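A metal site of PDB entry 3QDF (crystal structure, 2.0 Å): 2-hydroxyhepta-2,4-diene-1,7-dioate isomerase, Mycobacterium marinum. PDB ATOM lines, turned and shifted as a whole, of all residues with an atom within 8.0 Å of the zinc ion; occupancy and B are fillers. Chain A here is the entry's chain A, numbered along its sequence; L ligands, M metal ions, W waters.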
ATOM      1  N   CYS A  69      -2.268  15.345  -8.768  1.00  0.00           N
ATOM      2  CA  CYS A  69      -0.849  15.094  -8.681  1.00  0.00           C
ATOM      3  C   CYS A  69      -0.476  13.696  -9.118  1.00  0.00           C
ATOM      4  O   CYS A  69      -1.244  12.734  -8.944  1.00  0.00           O
ATOM      5  CB  CYS A  69      -0.357  15.258  -7.255  1.00  0.00           C
ATOM      6  SG  CYS A  69      -0.801  16.781  -6.469  1.00  0.00           S
ATOM      7  N   VAL A  70       0.751  13.559  -9.606  1.00  0.00           N
ATOM      8  CA  VAL A  70       1.238  12.287 -10.086  1.00  0.00           C
ATOM      9  C   VAL A  70       2.295  11.779  -9.089  1.00  0.00           C
ATOM     10  O   VAL A  70       3.148  12.537  -8.645  1.00  0.00           O
ATOM     11  CB  VAL A  70       1.785  12.435 -11.528  1.00  0.00           C
ATOM     12  CG1 VAL A  70       2.362  11.112 -12.035  1.00  0.00           C
ATOM     13  CG2 VAL A  70       0.672  12.926 -12.482  1.00  0.00           C
ATOM     14  N   GLY A  71       2.195  10.500  -8.721  1.00  0.00           N
ATOM     15  CA  GLY A  71       3.223   9.846  -7.899  1.00  0.00           C
ATOM     16  C   GLY A  71       4.552   9.653  -8.606  1.00  0.00           C
ATOM     17  O   GLY A  71       5.049  10.555  -9.289  1.00  0.00           O
ATOM     18  N   LYS A  72       5.165   8.491  -8.389  1.00  0.00           N
ATOM     19  CA  LYS A  72       6.392   8.078  -9.032  1.00  0.00           C
ATOM     20  C   LYS A  72       6.432   8.345 -10.539  1.00  0.00           C
ATOM     21  O   LYS A  72       5.834   7.593 -11.314  1.00  0.00           O
ATOM     22  CB  LYS A  72       6.543   6.563  -8.799  1.00  0.00           C
ATOM     23  N   ASN A  73       7.126   9.404 -10.972  1.00  0.00           N
ATOM     24  CA  ASN A  73       7.181   9.764 -12.406  1.00  0.00           C
ATOM     25  C   ASN A  73       8.569  10.084 -12.994  1.00  0.00           C
ATOM     26  O   ASN A  73       8.664  10.660 -14.074  1.00  0.00           O
ATOM     27  CB  ASN A  73       6.183  10.903 -12.726  1.00  0.00           C
ATOM     28  CG  ASN A  73       5.797  10.952 -14.203  1.00  0.00           C
ATOM     29  OD1 ASN A  73       5.655   9.917 -14.869  1.00  0.00           O
ATOM     30  ND2 ASN A  73       5.603  12.152 -14.719  1.00  0.00           N
ATOM     31  N   PHE A  95      -3.258  11.353  -7.236  1.00  0.00           N
ATOM     32  CA  PHE A  95      -3.844  11.699  -5.950  1.00  0.00           C
ATOM     33  C   PHE A  95      -4.204  13.170  -5.968  1.00  0.00           C
ATOM     34  O   PHE A  95      -3.893  13.847  -6.927  1.00  0.00           O
ATOM     35  CB  PHE A  95      -2.913  11.361  -4.780  1.00  0.00           C
ATOM     36  CG  PHE A  95      -1.568  12.069  -4.827  1.00  0.00           C
ATOM     37  CD1 PHE A  95      -0.508  11.512  -5.539  1.00  0.00           C
ATOM     38  CD2 PHE A  95      -1.364  13.277  -4.144  1.00  0.00           C
ATOM     39  CE1 PHE A  95       0.752  12.146  -5.574  1.00  0.00           C
ATOM     40  CE2 PHE A  95      -0.100  13.928  -4.162  1.00  0.00           C
ATOM     41  CZ  PHE A  95       0.951  13.364  -4.883  1.00  0.00           C
ATOM     42  N   LYS A  97      -4.419  17.012  -3.842  1.00  0.00           N
ATOM     43  CA  LYS A  97      -4.181  17.928  -2.758  1.00  0.00           C
ATOM     44  C   LYS A  97      -5.330  18.937  -2.769  1.00  0.00           C
ATOM     45  O   LYS A  97      -5.767  19.348  -3.854  1.00  0.00           O
ATOM     46  CB  LYS A  97      -2.836  18.623  -2.915  1.00  0.00           C
ATOM     47  CG  LYS A  97      -1.625  17.676  -2.669  1.00  0.00           C
ATOM     48  CD  LYS A  97      -0.323  18.291  -3.231  1.00  0.00           C
ATOM     49  CE  LYS A  97       0.360  19.267  -2.214  1.00  0.00           C
ATOM     50  NZ  LYS A  97       1.265  18.547  -1.210  1.00  0.00           N
ATOM     51  N   PHE A 120      10.201  18.270   1.058  1.00  0.00           N
ATOM     52  CA  PHE A 120       9.907  19.059  -0.132  1.00  0.00           C
ATOM     53  C   PHE A 120       9.830  18.096  -1.322  1.00  0.00           C
ATOM     54  O   PHE A 120      10.373  16.988  -1.262  1.00  0.00           O
ATOM     55  CB  PHE A 120      10.992  20.117  -0.376  1.00  0.00           C
ATOM     56  CG  PHE A 120      12.349  19.511  -0.657  1.00  0.00           C
ATOM     57  CD1 PHE A 120      12.661  19.044  -1.927  1.00  0.00           C
ATOM     58  CD2 PHE A 120      13.281  19.334   0.367  1.00  0.00           C
ATOM     59  CE1 PHE A 120      13.887  18.456  -2.186  1.00  0.00           C
ATOM     60  CE2 PHE A 120      14.511  18.740   0.120  1.00  0.00           C
ATOM     61  CZ  PHE A 120      14.819  18.302  -1.167  1.00  0.00           C
ATOM     62  N   GLU A 121       9.160  18.509  -2.386  1.00  0.00           N
ATOM     63  CA  GLU A 121       9.239  17.808  -3.667  1.00  0.00           C
ATOM     64  C   GLU A 121       9.040  18.853  -4.744  1.00  0.00           C
ATOM     65  O   GLU A 121       7.934  19.315  -4.945  1.00  0.00           O
ATOM     66  CB  GLU A 121       8.134  16.739  -3.820  1.00  0.00           C
ATOM     67  CG  GLU A 121       8.203  15.536  -2.848  1.00  0.00           C
ATOM     68  CD  GLU A 121       7.208  14.439  -3.216  1.00  0.00           C
ATOM     69  OE1 GLU A 121       7.322  13.287  -2.713  1.00  0.00           O
ATOM     70  OE2 GLU A 121       6.313  14.705  -4.032  1.00  0.00           O
ATOM     71  N   GLY A 122      10.119  19.197  -5.451  1.00  0.00           N
ATOM     72  CA  GLY A 122      10.051  20.151  -6.565  1.00  0.00           C
ATOM     73  C   GLY A 122       9.438  19.487  -7.768  1.00  0.00           C
ATOM     74  O   GLY A 122       9.840  18.383  -8.133  1.00  0.00           O
ATOM     75  N   GLU A 123       8.446  20.161  -8.387  1.00  0.00           N
ATOM     76  CA  GLU A 123       7.719  19.584  -9.510  1.00  0.00           C
ATOM     77  C   GLU A 123       7.303  20.620 -10.553  1.00  0.00           C
ATOM     78  O   GLU A 123       6.889  21.747 -10.213  1.00  0.00           O
ATOM     79  CB  GLU A 123       6.442  18.861  -9.027  1.00  0.00           C
ATOM     80  CG  GLU A 123       6.699  17.965  -7.826  1.00  0.00           C
ATOM     81  CD  GLU A 123       5.669  16.885  -7.596  1.00  0.00           C
ATOM     82  OE1 GLU A 123       4.645  16.759  -8.344  1.00  0.00           O
ATOM     83  OE2 GLU A 123       5.886  16.133  -6.621  1.00  0.00           O
ATOM     84  N   GLY A 150       5.531  23.737  -8.680  1.00  0.00           N
ATOM     85  CA  GLY A 150       4.902  23.317  -7.449  1.00  0.00           C
ATOM     86  C   GLY A 150       5.898  22.676  -6.499  1.00  0.00           C
ATOM     87  O   GLY A 150       6.934  22.116  -6.924  1.00  0.00           O
ATOM     88  N   ASN A 151       5.585  22.783  -5.204  1.00  0.00           N
ATOM     89  CA  ASN A 151       6.310  22.074  -4.157  1.00  0.00           C
ATOM     90  C   ASN A 151       5.329  21.135  -3.474  1.00  0.00           C
ATOM     91  O   ASN A 151       4.484  21.562  -2.656  1.00  0.00           O
ATOM     92  CB  ASN A 151       6.916  23.050  -3.123  1.00  0.00           C
ATOM     93  CG  ASN A 151       7.912  22.387  -2.168  1.00  0.00           C
ATOM     94  OD1 ASN A 151       7.933  21.170  -2.043  1.00  0.00           O
ATOM     95  ND2 ASN A 151       8.724  23.190  -1.489  1.00  0.00           N
ATOM     96  N   ASP A 152       5.425  19.838  -3.810  1.00  0.00           N
ATOM     97  CA  ASP A 152       4.525  18.835  -3.234  1.00  0.00           C
ATOM     98  C   ASP A 152       4.954  18.440  -1.815  1.00  0.00           C
ATOM     99  O   ASP A 152       5.525  17.343  -1.572  1.00  0.00           O
ATOM    100  CB  ASP A 152       4.460  17.608  -4.153  1.00  0.00           C
ATOM    101  CG  ASP A 152       3.473  16.564  -3.663  1.00  0.00           C
ATOM    102  OD1 ASP A 152       2.618  16.902  -2.816  1.00  0.00           O
ATOM    103  OD2 ASP A 152       3.543  15.418  -4.134  1.00  0.00           O
ATOM    104  N   VAL A 153       4.699  19.319  -0.865  1.00  0.00           N
ATOM    105  CA  VAL A 153       5.161  19.079   0.513  1.00  0.00           C
ATOM    106  C   VAL A 153       4.447  17.855   1.112  1.00  0.00           C
ATOM    107  O   VAL A 153       3.217  17.709   0.974  1.00  0.00           O
ATOM    108  CB  VAL A 153       5.045  20.350   1.375  1.00  0.00           C
ATOM    109  CG1 VAL A 153       5.637  20.115   2.736  1.00  0.00           C
ATOM    110  CG2 VAL A 153       5.766  21.501   0.689  1.00  0.00           C
ATOM    111  N   SER A 154       5.218  16.974   1.757  1.00  0.00           N
ATOM    112  CA  SER A 154       4.741  15.645   2.133  1.00  0.00           C
ATOM    113  C   SER A 154       5.266  15.207   3.503  1.00  0.00           C
ATOM    114  O   SER A 154       6.498  15.105   3.704  1.00  0.00           O
ATOM    115  CB  SER A 154       5.187  14.610   1.079  1.00  0.00           C
ATOM    116  OG  SER A 154       4.934  15.069  -0.244  1.00  0.00           O
ATOM    117  N   ARG A 156       6.091  12.374   5.472  1.00  0.00           N
ATOM    118  CA  ARG A 156       6.418  10.954   5.191  1.00  0.00           C
ATOM    119  C   ARG A 156       5.929   9.947   6.245  1.00  0.00           C
ATOM    120  O   ARG A 156       5.520   8.840   5.900  1.00  0.00           O
ATOM    121  CB  ARG A 156       7.925  10.759   4.983  1.00  0.00           C
ATOM    122  CG  ARG A 156       8.549  11.517   3.793  1.00  0.00           C
ATOM    123  CD  ARG A 156       7.892  11.221   2.450  1.00  0.00           C
ATOM    124  NE  ARG A 156       8.665  11.749   1.324  1.00  0.00           N
ATOM    125  CZ  ARG A 156       8.170  12.033   0.110  1.00  0.00           C
ATOM    126  NH1 ARG A 156       6.884  11.845  -0.185  1.00  0.00           N
ATOM    127  NH2 ARG A 156       8.990  12.513  -0.829  1.00  0.00           N
ATOM    128  N   TRP A 165      -2.229   8.755   0.665  1.00  0.00           N
ATOM    129  CA  TRP A 165      -1.291   9.859   0.743  1.00  0.00           C
ATOM    130  C   TRP A 165      -1.977  11.176   1.063  1.00  0.00           C
ATOM    131  O   TRP A 165      -1.303  12.179   1.275  1.00  0.00           O
ATOM    132  CB  TRP A 165      -0.511  10.003  -0.577  1.00  0.00           C
ATOM    133  CG  TRP A 165       0.356   8.815  -0.927  1.00  0.00           C
ATOM    134  CD1 TRP A 165       0.806   7.820  -0.076  1.00  0.00           C
ATOM    135  CD2 TRP A 165       0.897   8.492  -2.219  1.00  0.00           C
ATOM    136  NE1 TRP A 165       1.565   6.900  -0.764  1.00  0.00           N
ATOM    137  CE2 TRP A 165       1.647   7.289  -2.080  1.00  0.00           C
ATOM    138  CE3 TRP A 165       0.821   9.101  -3.476  1.00  0.00           C
ATOM    139  CZ2 TRP A 165       2.314   6.687  -3.175  1.00  0.00           C
ATOM    140  CZ3 TRP A 165       1.488   8.500  -4.561  1.00  0.00           C
ATOM    141  CH2 TRP A 165       2.223   7.308  -4.394  1.00  0.00           C
ATOM    142  N   LYS A 169      -0.057  14.780   2.369  1.00  0.00           N
ATOM    143  CA  LYS A 169       0.180  15.806   1.353  1.00  0.00           C
ATOM    144  C   LYS A 169      -0.805  16.987   1.383  1.00  0.00           C
ATOM    145  O   LYS A 169      -0.714  17.905   0.559  1.00  0.00           O
ATOM    146  CB  LYS A 169       0.218  15.153  -0.031  1.00  0.00           C
ATOM    147  CG  LYS A 169       1.533  14.408  -0.274  1.00  0.00           C
ATOM    148  CD  LYS A 169       1.381  13.383  -1.373  1.00  0.00           C
ATOM    149  CE  LYS A 169       2.670  12.623  -1.624  1.00  0.00           C
ATOM    150  NZ  LYS A 169       3.785  13.501  -2.074  1.00  0.00           N
ATOM    151  N   LEU A 233       0.358  18.608 -10.626  1.00  0.00           N
ATOM    152  CA  LEU A 233       1.776  18.397 -10.262  1.00  0.00           C
ATOM    153  C   LEU A 233       2.263  17.086 -10.866  1.00  0.00           C
ATOM    154  O   LEU A 233       1.700  16.014 -10.579  1.00  0.00           O
ATOM    155  CB  LEU A 233       1.955  18.390  -8.750  1.00  0.00           C
ATOM    156  CG  LEU A 233       1.446  19.574  -7.904  1.00  0.00           C
ATOM    157  CD1 LEU A 233       1.958  19.379  -6.443  1.00  0.00           C
ATOM    158  CD2 LEU A 233       1.877  20.925  -8.480  1.00  0.00           C
ATOM    159  N   THR A 234       3.326  17.156 -11.638  1.00  0.00           N
ATOM    160  CA  THR A 234       3.721  16.062 -12.538  1.00  0.00           C
ATOM    161  C   THR A 234       4.759  15.079 -11.974  1.00  0.00           C
ATOM    162  O   THR A 234       5.283  14.225 -12.705  1.00  0.00           O
ATOM    163  CB  THR A 234       4.189  16.593 -13.880  1.00  0.00           C
ATOM    164  OG1 THR A 234       5.415  17.301 -13.717  1.00  0.00           O
ATOM    165  CG2 THR A 234       3.131  17.520 -14.494  1.00  0.00           C
ATOM    166  N   GLY A 235       5.046  15.190 -10.677  1.00  0.00           N
ATOM    167  CA  GLY A 235       5.950  14.245 -10.004  1.00  0.00           C
ATOM    168  C   GLY A 235       7.282  14.908  -9.725  1.00  0.00           C
ATOM    169  O   GLY A 235       7.569  15.960 -10.295  1.00  0.00           O
ATOM    170  N   THR A 236       8.067  14.303  -8.852  1.00  0.00           N
ATOM    171  CA  THR A 236       9.328  14.882  -8.435  1.00  0.00           C
ATOM    172  C   THR A 236      10.490  13.934  -8.784  1.00  0.00           C
ATOM    173  O   THR A 236      10.333  12.685  -8.711  1.00  0.00           O
ATOM    174  CB  THR A 236       9.315  15.204  -6.908  1.00  0.00           C
ATOM    175  OG1 THR A 236      10.342  16.158  -6.590  1.00  0.00           O
ATOM    176  CG2 THR A 236       9.513  13.926  -6.048  1.00  0.00           C
ATOM    177  N   PRO A 237      11.656  14.505  -9.188  1.00  0.00           N
ATOM    178  CA  PRO A 237      12.863  13.690  -9.400  1.00  0.00           C
ATOM    179  C   PRO A 237      13.511  13.170  -8.110  1.00  0.00           C
ATOM    180  O   PRO A 237      13.040  13.463  -7.003  1.00  0.00           O
ATOM    181  CB  PRO A 237      13.835  14.643 -10.107  1.00  0.00           C
ATOM    182  CG  PRO A 237      13.303  16.024  -9.846  1.00  0.00           C
ATOM    183  CD  PRO A 237      11.837  15.903  -9.661  1.00  0.00           C
ATOM    184  N   VAL A 240      14.634  13.944  -3.025  1.00  0.00           N
ATOM    185  CA  VAL A 240      13.691  14.439  -1.999  1.00  0.00           C
ATOM    186  C   VAL A 240      14.360  14.391  -0.634  1.00  0.00           C
ATOM    187  O   VAL A 240      15.186  13.526  -0.390  1.00  0.00           O
ATOM    188  CB  VAL A 240      12.329  13.650  -1.966  1.00  0.00           C
ATOM    189  CG1 VAL A 240      11.531  13.958  -3.207  1.00  0.00           C
ATOM    190  CG2 VAL A 240      12.554  12.105  -1.825  1.00  0.00           C
HETATM  191  C1  LIG L   1       4.519  11.926  -4.956  1.00  0.00           C
HETATM  192  O1  LIG L   1       5.199  12.656  -5.994  1.00  0.00           O
HETATM  193  C2  LIG L   1       5.362  10.803  -4.328  1.00  0.00           C
HETATM  194  O2  LIG L   1       5.195  10.788  -2.889  1.00  0.00           O
HETATM  195 ZN    ZN M   1       4.780  14.726  -5.711  1.00  0.00          ZN
HETATM  196  O   HOH W   1       3.209  14.876  -7.346  1.00  0.00           O
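Water W1 bridges OE1 of Glu 123 (2.6 Å) and O of Val 70 (2.7 Å).
The side-chain carboxylate (OE1) of Glu 123 lies within hydrogen-bond range of the backbone NH (N) of Gly 235 (2.8 Å).
The side-chain carboxylate (OD1) of Asp 152 is in salt-bridge range of the side-chain amino group (NZ) of Lys 169, 3.7 Å away.
The side-chain hydroxyl (OG) of Ser 154 is in hydrogen-bond range of the backbone carbonyl oxygen (O) of Asp 152 (2.7 Å).
NZ of Lys 97 is in salt-bridge range of OD1 of Asp 152 (2.7 Å).
The side-chain carboxylate (OE1) of Glu 121 is in salt-bridge range of the side-chain amino group (NZ) of Lys 169 (3.6 Å).
NH2 of Arg 156 is in salt-bridge range of OE1 of Glu 121, 2.6 Å away.
N of Glu 121 sits at hydrogen-bond distance from OD1 of Asn 151.
The side-chain amino group (NZ) of Lys 169 sits at hydrogen-bond distance from the side-chain hydroxyl (OG) of Ser 154, at 2.7 Å.
The zinc ion is bound by OE2 of Glu 123 (2.0 Å), OD2 of Asp 152 (2.1 Å), O1 of the ligand (2.1 Å), water W1 (2.3 Å) and OE2 of Glu 121 (2.3 Å).
The zinc ion has five donor atoms within binding distance.
Merely in contact with the zinc ion: Lys 169.
The nearest printed residue that does not touch the zinc ion is Val 70 (4.01 Å).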
